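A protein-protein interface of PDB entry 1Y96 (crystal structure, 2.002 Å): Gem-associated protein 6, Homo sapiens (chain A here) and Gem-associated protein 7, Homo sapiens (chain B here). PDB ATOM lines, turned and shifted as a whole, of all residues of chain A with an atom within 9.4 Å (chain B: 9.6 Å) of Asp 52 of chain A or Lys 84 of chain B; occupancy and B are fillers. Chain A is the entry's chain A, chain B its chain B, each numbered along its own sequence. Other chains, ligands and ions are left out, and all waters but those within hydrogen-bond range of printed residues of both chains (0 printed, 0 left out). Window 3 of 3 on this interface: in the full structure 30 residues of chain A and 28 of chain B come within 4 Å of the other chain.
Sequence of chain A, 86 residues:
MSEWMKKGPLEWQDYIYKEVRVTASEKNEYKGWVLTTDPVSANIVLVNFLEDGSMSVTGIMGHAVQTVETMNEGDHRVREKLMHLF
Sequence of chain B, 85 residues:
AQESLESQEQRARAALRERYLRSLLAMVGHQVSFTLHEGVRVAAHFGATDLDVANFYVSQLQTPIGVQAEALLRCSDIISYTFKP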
ATOM      1  N   LEU A  46      -2.247  -0.086 -13.494  1.00  0.00           N
ATOM      2  CA  LEU A  46      -0.862   0.406 -13.600  1.00  0.00           C
ATOM      3  C   LEU A  46       0.049  -0.123 -12.510  1.00  0.00           C
ATOM      4  O   LEU A  46      -0.367  -0.264 -11.366  1.00  0.00           O
ATOM      5  CB  LEU A  46      -0.840   1.934 -13.532  1.00  0.00           C
ATOM      6  CG  LEU A  46      -1.686   2.701 -14.536  1.00  0.00           C
ATOM      7  CD1 LEU A  46      -1.546   4.210 -14.347  1.00  0.00           C
ATOM      8  CD2 LEU A  46      -1.333   2.308 -15.947  1.00  0.00           C
ATOM      9  N   ASN A  48       3.680   0.720 -10.570  1.00  0.00           N
ATOM     10  CA  ASN A  48       4.669   1.765 -10.286  1.00  0.00           C
ATOM     11  C   ASN A  48       5.819   1.202  -9.510  1.00  0.00           C
ATOM     12  O   ASN A  48       5.626   0.543  -8.492  1.00  0.00           O
ATOM     13  CB  ASN A  48       4.065   2.902  -9.484  1.00  0.00           C
ATOM     14  CG  ASN A  48       3.224   3.803 -10.320  1.00  0.00           C
ATOM     15  OD1 ASN A  48       2.023   3.569 -10.476  1.00  0.00           O
ATOM     16  ND2 ASN A  48       3.842   4.840 -10.888  1.00  0.00           N
ATOM     17  N   PHE A  49       7.021   1.449 -10.020  1.00  0.00           N
ATOM     18  CA  PHE A  49       8.266   1.217  -9.299  1.00  0.00           C
ATOM     19  C   PHE A  49       8.640   2.551  -8.638  1.00  0.00           C
ATOM     20  O   PHE A  49       9.008   3.531  -9.307  1.00  0.00           O
ATOM     21  CB  PHE A  49       9.340   0.736 -10.273  1.00  0.00           C
ATOM     22  CG  PHE A  49       8.959  -0.503 -11.045  1.00  0.00           C
ATOM     23  CD1 PHE A  49       8.442  -0.405 -12.332  1.00  0.00           C
ATOM     24  CD2 PHE A  49       9.148  -1.765 -10.501  1.00  0.00           C
ATOM     25  CE1 PHE A  49       8.098  -1.549 -13.064  1.00  0.00           C
ATOM     26  CE2 PHE A  49       8.813  -2.913 -11.221  1.00  0.00           C
ATOM     27  CZ  PHE A  49       8.288  -2.807 -12.503  1.00  0.00           C
ATOM     28  N   LEU A  50       8.467   2.609  -7.329  1.00  0.00           N
ATOM     29  CA  LEU A  50       8.484   3.871  -6.597  1.00  0.00           C
ATOM     30  C   LEU A  50       9.907   4.219  -6.128  1.00  0.00           C
ATOM     31  O   LEU A  50      10.784   3.369  -6.118  1.00  0.00           O
ATOM     32  CB  LEU A  50       7.519   3.788  -5.395  1.00  0.00           C
ATOM     33  CG  LEU A  50       6.023   3.551  -5.699  1.00  0.00           C
ATOM     34  CD1 LEU A  50       5.262   3.258  -4.408  1.00  0.00           C
ATOM     35  CD2 LEU A  50       5.407   4.733  -6.410  1.00  0.00           C
ATOM     36  N   GLU A  51      10.089   5.471  -5.721  1.00  0.00           N
ATOM     37  CA  GLU A  51      11.400   6.034  -5.337  1.00  0.00           C
ATOM     38  C   GLU A  51      12.099   5.310  -4.204  1.00  0.00           C
ATOM     39  O   GLU A  51      13.316   5.435  -4.059  1.00  0.00           O
ATOM     40  CB  GLU A  51      11.233   7.447  -4.806  1.00  0.00           C
ATOM     41  CG  GLU A  51      10.814   8.524  -5.769  1.00  0.00           C
ATOM     42  CD  GLU A  51      10.233   9.688  -4.985  1.00  0.00           C
ATOM     43  OE1 GLU A  51       9.013   9.932  -5.082  1.00  0.00           O
ATOM     44  OE2 GLU A  51      11.000  10.342  -4.233  1.00  0.00           O
ATOM     45  N   ASP A  52      11.329   4.635  -3.351  1.00  0.00           N
ATOM     46  CA  ASP A  52      11.894   3.927  -2.205  1.00  0.00           C
ATOM     47  C   ASP A  52      12.197   2.466  -2.486  1.00  0.00           C
ATOM     48  O   ASP A  52      12.537   1.714  -1.586  1.00  0.00           O
ATOM     49  CB  ASP A  52      11.013   4.111  -0.956  1.00  0.00           C
ATOM     50  CG  ASP A  52       9.630   3.453  -1.075  1.00  0.00           C
ATOM     51  OD1 ASP A  52       9.236   3.041  -2.192  1.00  0.00           O
ATOM     52  OD2 ASP A  52       8.878   3.310  -0.076  1.00  0.00           O
ATOM     53  N   GLY A  53      12.088   2.058  -3.747  1.00  0.00           N
ATOM     54  CA  GLY A  53      12.342   0.684  -4.124  1.00  0.00           C
ATOM     55  C   GLY A  53      11.186  -0.300  -3.954  1.00  0.00           C
ATOM     56  O   GLY A  53      11.348  -1.486  -4.233  1.00  0.00           O
ATOM     57  N   SER A  54      10.035   0.172  -3.492  1.00  0.00           N
ATOM     58  CA  SER A  54       8.864  -0.696  -3.331  1.00  0.00           C
ATOM     59  C   SER A  54       8.032  -0.629  -4.602  1.00  0.00           C
ATOM     60  O   SER A  54       8.302   0.183  -5.489  1.00  0.00           O
ATOM     61  CB  SER A  54       8.032  -0.283  -2.116  1.00  0.00           C
ATOM     62  OG  SER A  54       7.411   0.980  -2.303  1.00  0.00           O
ATOM     63  N   MET A  55       7.013  -1.470  -4.690  1.00  0.00           N
ATOM     64  CA  MET A  55       6.187  -1.510  -5.891  1.00  0.00           C
ATOM     65  C   MET A  55       4.709  -1.384  -5.545  1.00  0.00           C
ATOM     66  O   MET A  55       4.249  -2.062  -4.634  1.00  0.00           O
ATOM     67  CB  MET A  55       6.460  -2.814  -6.606  1.00  0.00           C
ATOM     68  CG  MET A  55       5.993  -2.815  -8.038  1.00  0.00           C
ATOM     69  SD  MET A  55       6.146  -4.460  -8.729  1.00  0.00           S
ATOM     70  CE  MET A  55       4.838  -5.293  -7.795  1.00  0.00           C
ATOM     71  N   SER A  56       3.988  -0.490  -6.234  1.00  0.00           N
ATOM     72  CA  SER A  56       2.542  -0.403  -6.095  1.00  0.00           C
ATOM     73  C   SER A  56       1.823  -0.832  -7.374  1.00  0.00           C
ATOM     74  O   SER A  56       2.401  -0.820  -8.468  1.00  0.00           O
ATOM     75  CB  SER A  56       2.088   1.002  -5.683  1.00  0.00           C
ATOM     76  OG  SER A  56       2.183   1.929  -6.750  1.00  0.00           O
ATOM     77  N   VAL A  57       0.549  -1.193  -7.193  1.00  0.00           N
ATOM     78  CA  VAL A  57      -0.373  -1.520  -8.271  1.00  0.00           C
ATOM     79  C   VAL A  57      -1.609  -0.657  -8.078  1.00  0.00           C
ATOM     80  O   VAL A  57      -2.185  -0.598  -6.972  1.00  0.00           O
ATOM     81  CB  VAL A  57      -0.735  -2.998  -8.230  1.00  0.00           C
ATOM     82  CG1 VAL A  57      -1.870  -3.342  -9.251  1.00  0.00           C
ATOM     83  CG2 VAL A  57       0.499  -3.862  -8.476  1.00  0.00           C
ATOM     84  N   THR A  58      -2.034   0.000  -9.148  1.00  0.00           N
ATOM     85  CA  THR A  58      -3.131   0.956  -9.105  1.00  0.00           C
ATOM     86  C   THR A  58      -4.158   0.648 -10.202  1.00  0.00           C
ATOM     87  O   THR A  58      -3.798   0.483 -11.369  1.00  0.00           O
ATOM     88  CB  THR A  58      -2.578   2.382  -9.297  1.00  0.00           C
ATOM     89  OG1 THR A  58      -1.695   2.697  -8.210  1.00  0.00           O
ATOM     90  CG2 THR A  58      -3.672   3.439  -9.232  1.00  0.00           C
ATOM     91  N   PHE A  86       2.703 -11.591 -10.866  1.00  0.00           N
ATOM     92  CA  PHE A  86       1.501 -12.417 -10.633  1.00  0.00           C
ATOM     93  C   PHE A  86       1.468 -13.679 -11.498  1.00  0.00           C
ATOM     94  O   PHE A  86       2.208 -14.635 -11.249  1.00  0.00           O
ATOM     95  CB  PHE A  86       0.202 -11.615 -10.840  1.00  0.00           C
ATOM     96  CG  PHE A  86       0.190 -10.256 -10.177  1.00  0.00           C
ATOM     97  CD1 PHE A  86      -0.455  -9.185 -10.789  1.00  0.00           C
ATOM     98  CD2 PHE A  86       0.809 -10.047  -8.943  1.00  0.00           C
ATOM     99  CE1 PHE A  86      -0.477  -7.932 -10.187  1.00  0.00           C
ATOM    100  CE2 PHE A  86       0.788  -8.795  -8.341  1.00  0.00           C
ATOM    101  CZ  PHE A  86       0.145  -7.740  -8.962  1.00  0.00           C
ATOM    102  N   ALA B  26      -4.523 -11.184  -6.629  1.00  0.00           N
ATOM    103  CA  ALA B  26      -3.291 -10.815  -5.906  1.00  0.00           C
ATOM    104  C   ALA B  26      -3.495  -9.750  -4.826  1.00  0.00           C
ATOM    105  O   ALA B  26      -2.661  -9.602  -3.926  1.00  0.00           O
ATOM    106  CB  ALA B  26      -2.238 -10.333  -6.881  1.00  0.00           C
ATOM    107  N   MET B  27      -4.572  -8.978  -4.960  1.00  0.00           N
ATOM    108  CA  MET B  27      -4.931  -7.944  -4.003  1.00  0.00           C
ATOM    109  C   MET B  27      -5.682  -8.464  -2.774  1.00  0.00           C
ATOM    110  O   MET B  27      -5.786  -7.743  -1.792  1.00  0.00           O
ATOM    111  CB  MET B  27      -5.765  -6.857  -4.720  1.00  0.00           C
ATOM    112  CG  MET B  27      -5.756  -5.517  -4.037  1.00  0.00           C
ATOM    113  SD  MET B  27      -6.730  -4.306  -4.901  1.00  0.00           S
ATOM    114  CE  MET B  27      -6.000  -3.793  -5.531  1.00  0.00           C
ATOM    115  N   VAL B  28      -6.205  -9.696  -2.822  1.00  0.00           N
ATOM    116  CA  VAL B  28      -6.979 -10.260  -1.708  1.00  0.00           C
ATOM    117  C   VAL B  28      -6.149 -10.229  -0.403  1.00  0.00           C
ATOM    118  O   VAL B  28      -4.984 -10.599  -0.402  1.00  0.00           O
ATOM    119  CB  VAL B  28      -7.474 -11.715  -2.030  1.00  0.00           C
ATOM    120  CG1 VAL B  28      -8.005 -12.422  -0.771  1.00  0.00           C
ATOM    121  CG2 VAL B  28      -8.545 -11.695  -3.150  1.00  0.00           C
ATOM    122  N   GLY B  29      -6.752  -9.730   0.675  1.00  0.00           N
ATOM    123  CA  GLY B  29      -6.116  -9.643   1.980  1.00  0.00           C
ATOM    124  C   GLY B  29      -5.162  -8.466   2.201  1.00  0.00           C
ATOM    125  O   GLY B  29      -4.600  -8.335   3.284  1.00  0.00           O
ATOM    126  N   HIS B  30      -4.949  -7.617   1.201  1.00  0.00           N
ATOM    127  CA  HIS B  30      -4.074  -6.466   1.389  1.00  0.00           C
ATOM    128  C   HIS B  30      -4.893  -5.253   1.716  1.00  0.00           C
ATOM    129  O   HIS B  30      -6.037  -5.145   1.300  1.00  0.00           O
ATOM    130  CB  HIS B  30      -3.291  -6.145   0.118  1.00  0.00           C
ATOM    131  CG  HIS B  30      -2.294  -7.186  -0.260  1.00  0.00           C
ATOM    132  ND1 HIS B  30      -0.934  -6.975  -0.174  1.00  0.00           N
ATOM    133  CD2 HIS B  30      -2.456  -8.430  -0.764  1.00  0.00           C
ATOM    134  CE1 HIS B  30      -0.299  -8.050  -0.612  1.00  0.00           C
ATOM    135  NE2 HIS B  30      -1.202  -8.945  -0.981  1.00  0.00           N
ATOM    136  N   GLN B  31      -4.272  -4.317   2.427  1.00  0.00           N
ATOM    137  CA  GLN B  31      -4.856  -3.013   2.659  1.00  0.00           C
ATOM    138  C   GLN B  31      -4.787  -2.241   1.350  1.00  0.00           C
ATOM    139  O   GLN B  31      -3.733  -2.183   0.698  1.00  0.00           O
ATOM    140  CB  GLN B  31      -4.071  -2.273   3.748  1.00  0.00           C
ATOM    141  CG  GLN B  31      -4.584  -0.870   4.036  1.00  0.00           C
ATOM    142  CD  GLN B  31      -5.492  -0.824   5.242  1.00  0.00           C
ATOM    143  OE1 GLN B  31      -5.270  -0.047   6.179  1.00  0.00           O
ATOM    144  NE2 GLN B  31      -6.524  -1.643   5.222  1.00  0.00           N
ATOM    145  N   VAL B  32      -5.911  -1.682   0.943  1.00  0.00           N
ATOM    146  CA  VAL B  32      -5.936  -0.848  -0.227  1.00  0.00           C
ATOM    147  C   VAL B  32      -6.525   0.510   0.121  1.00  0.00           C
ATOM    148  O   VAL B  32      -7.370   0.636   1.009  1.00  0.00           O
ATOM    149  CB  VAL B  32      -6.569  -1.555  -1.505  1.00  0.00           C
ATOM    150  CG1 VAL B  32      -6.877  -3.042  -1.302  1.00  0.00           C
ATOM    151  CG2 VAL B  32      -7.697  -0.790  -2.133  1.00  0.00           C
ATOM    152  N   SER B  33      -6.033   1.510  -0.582  1.00  0.00           N
ATOM    153  CA  SER B  33      -6.431   2.889  -0.415  1.00  0.00           C
ATOM    154  C   SER B  33      -7.246   3.284  -1.633  1.00  0.00           C
ATOM    155  O   SER B  33      -6.774   3.203  -2.766  1.00  0.00           O
ATOM    156  CB  SER B  33      -5.160   3.776  -0.257  1.00  0.00           C
ATOM    157  OG  SER B  33      -5.498   5.137  -0.454  1.00  0.00           O
ATOM    158  N   ALA B  44      -9.241   0.124   3.283  1.00  0.00           N
ATOM    159  CA  ALA B  44      -9.875  -1.119   3.693  1.00  0.00           C
ATOM    160  C   ALA B  44      -9.094  -2.318   3.170  1.00  0.00           C
ATOM    161  O   ALA B  44      -8.318  -2.184   2.229  1.00  0.00           O
ATOM    162  CB  ALA B  44     -11.280  -1.147   3.185  1.00  0.00           C
ATOM    163  N   TYR B  81      -7.967   2.824  -7.002  1.00  0.00           N
ATOM    164  CA  TYR B  81      -7.560   2.015  -5.855  1.00  0.00           C
ATOM    165  C   TYR B  81      -6.106   1.649  -5.998  1.00  0.00           C
ATOM    166  O   TYR B  81      -5.648   1.375  -7.095  1.00  0.00           O
ATOM    167  CB  TYR B  81      -8.412   0.738  -5.730  1.00  0.00           C
ATOM    168  CG  TYR B  81      -8.415  -0.194  -6.945  1.00  0.00           C
ATOM    169  CD1 TYR B  81      -7.512  -1.235  -7.049  1.00  0.00           C
ATOM    170  CD2 TYR B  81      -9.370  -0.058  -7.953  1.00  0.00           C
ATOM    171  CE1 TYR B  81      -7.515  -2.094  -8.150  1.00  0.00           C
ATOM    172  CE2 TYR B  81      -9.392  -0.917  -9.050  1.00  0.00           C
ATOM    173  CZ  TYR B  81      -8.465  -1.950  -9.133  1.00  0.00           C
ATOM    174  OH  TYR B  81      -8.464  -2.797 -10.221  1.00  0.00           O
ATOM    175  N   THR B  82      -5.367   1.633  -4.894  1.00  0.00           N
ATOM    176  CA  THR B  82      -3.958   1.296  -4.935  1.00  0.00           C
ATOM    177  C   THR B  82      -3.564   0.433  -3.765  1.00  0.00           C
ATOM    178  O   THR B  82      -4.101   0.560  -2.684  1.00  0.00           O
ATOM    179  CB  THR B  82      -3.064   2.581  -4.936  1.00  0.00           C
ATOM    180  OG1 THR B  82      -3.435   3.441  -6.026  1.00  0.00           O
ATOM    181  CG2 THR B  82      -1.651   2.238  -5.260  1.00  0.00           C
ATOM    182  N   PHE B  83      -2.614  -0.445  -3.990  1.00  0.00           N
ATOM    183  CA  PHE B  83      -2.037  -1.233  -2.929  1.00  0.00           C
ATOM    184  C   PHE B  83      -0.604  -1.606  -3.256  1.00  0.00           C
ATOM    185  O   PHE B  83      -0.132  -1.362  -4.361  1.00  0.00           O
ATOM    186  CB  PHE B  83      -2.889  -2.489  -2.686  1.00  0.00           C
ATOM    187  CG  PHE B  83      -2.613  -3.620  -3.613  1.00  0.00           C
ATOM    188  CD1 PHE B  83      -1.952  -4.750  -3.176  1.00  0.00           C
ATOM    189  CD2 PHE B  83      -3.039  -3.582  -4.928  1.00  0.00           C
ATOM    190  CE1 PHE B  83      -1.741  -5.802  -4.024  1.00  0.00           C
ATOM    191  CE2 PHE B  83      -2.804  -4.640  -5.778  1.00  0.00           C
ATOM    192  CZ  PHE B  83      -2.170  -5.749  -5.322  1.00  0.00           C
ATOM    193  N   LYS B  84       0.060  -2.250  -2.307  1.00  0.00           N
ATOM    194  CA  LYS B  84       1.445  -2.649  -2.461  1.00  0.00           C
ATOM    195  C   LYS B  84       1.587  -4.151  -2.258  1.00  0.00           C
ATOM    196  O   LYS B  84       1.406  -4.637  -1.160  1.00  0.00           O
ATOM    197  CB  LYS B  84       2.305  -1.908  -1.438  1.00  0.00           C
ATOM    198  CG  LYS B  84       2.564  -0.457  -1.774  1.00  0.00           C
ATOM    199  CD  LYS B  84       3.945  -0.019  -1.233  1.00  0.00           C
ATOM    200  CE  LYS B  84       4.140   1.469  -1.351  1.00  0.00           C
ATOM    201  NZ  LYS B  84       5.268   1.940  -0.495  1.00  0.00           N
ATOM    202  N   PRO B  85       1.920  -4.895  -3.300  1.00  0.00           N
ATOM    203  CA  PRO B  85       2.103  -6.343  -3.144  1.00  0.00           C
ATOM    204  C   PRO B  85       3.214  -6.707  -2.150  1.00  0.00           C
ATOM    205  O   PRO B  85       4.233  -6.006  -2.192  1.00  0.00           O
ATOM    206  CB  PRO B  85       2.459  -6.803  -4.553  1.00  0.00           C
ATOM    207  CG  PRO B  85       1.970  -5.734  -5.442  1.00  0.00           C
ATOM    208  CD  PRO B  85       2.135  -4.457  -4.690  1.00  0.00           C
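The side-chain amino group (NZ) of Lys 84 of chain B is in salt-bridge range of the side-chain carboxylate (OD2) of Asp 52 of chain A (3.9 Å). The side-chain hydroxyl of Ser 54 of chain A sits at hydrogen-bond distance from the side-chain amino group of Lys 84 of chain B (3.0 Å). O of Phe 83 of chain B sits at hydrogen-bond distance from N of Val 57 of chain A, 2.9 Å away. OG1 of Thr 58 of chain A sits at hydrogen-bond distance from OG1 of Thr 82 of chain B (2.9 Å).
O of Thr 58 of chain A is in hydrogen-bond range of N of Leu 46 of chain A. O of Ser 56 of chain A is in hydrogen-bond range of N of Asn 48 of chain A (2.9 Å). The side-chain carboxylate of Asp 52 of chain A sits at hydrogen-bond distance from the side-chain hydroxyl of Ser 54 of chain A. The backbone carbonyl oxygen (O) of Ala 26 of chain B sits at hydrogen-bond distance from a ring nitrogen (NE2) of His 30 of chain B (3.4 Å). The backbone carbonyl oxygen (O) of Lys 84 of chain B is in hydrogen-bond range of a ring nitrogen (ND1) of His 30 of chain B (3.5 Å). The backbone carbonyl oxygen of Ser 33 of chain B sits at hydrogen-bond distance from the backbone NH of Thr 82 of chain B (3.0 Å).
Among the printed residues, pairs that only touch across the chains: Met 55 of chain A with Pro 85 of chain B, Thr 58 of chain A with Tyr 81 of chain B, Val 57 of chain A with Thr 82 of chain B, Ser 56 of chain A with Phe 83 of chain B, Met 55 of chain A with Lys 84 of chain B, Phe 86 of chain A with Ala 26 of chain B, Leu 50 of chain A with Lys 84 of chain B, Val 57 of chain A with Pro 85 of chain B, Ser 56 of chain A with Thr 82 of chain B and Val 57 of chain A with Tyr 81 of chain B.
Asp 52 of chain A touches just one residue of chain B: Lys 84 (3.9 Å). Gly 53 of chain A touches none of the printed residues of chain B. Of chain B, only Lys 84 (3.0 Å) comes within 4 Å of Ser 54 of chain A. Of the printed residues of chain B, Ser 56 of chain A touches Thr 82 (3.96 Å) and Phe 83 (3.3 Å). Printed residues of chain B within 4 Å of Val 57 of chain A: Tyr 81 (3.99 Å), Thr 82 (3.3 Å), Phe 83 (2.9 Å) and Pro 85 (3.9 Å). Val 28 of chain B touches none of the printed residues of chain A. Of the printed residues of chain A, Tyr 81 of chain B touches Val 57 (3.99 Å) and Thr 58 (3.2 Å). Phe 83 of chain B touches just these residues of chain A: Ser 56 (3.3 Å) and Val 57 (2.9 Å). Lys 84 of chain B touches just these residues of chain A: Leu 50 (3.7 Å), Asp 52 (3.9 Å), Ser 54 (3.0 Å) and Met 55 (3.6 Å). The nearest residue of chain A that does not touch Lys 84 of chain B is Ser 56 of chain A (4.2 Å).
Of the 14 printed residues of chain B, 6 touch a printed residue of chain A. Hydrophobic or aromatic side chains of chain A within 4 Å of the printed part of chain B: Leu 50, Met 55, Val 57 and Phe 86. Among the printed residues, 14 pairs touch across the chains. Among the printed residues, Asp or Glu carboxylates within 4 Å of a Lys or Arg side-chain nitrogen of the other chain: Asp 52 of chain A with Lys 84 of chain B (3.9 Å).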
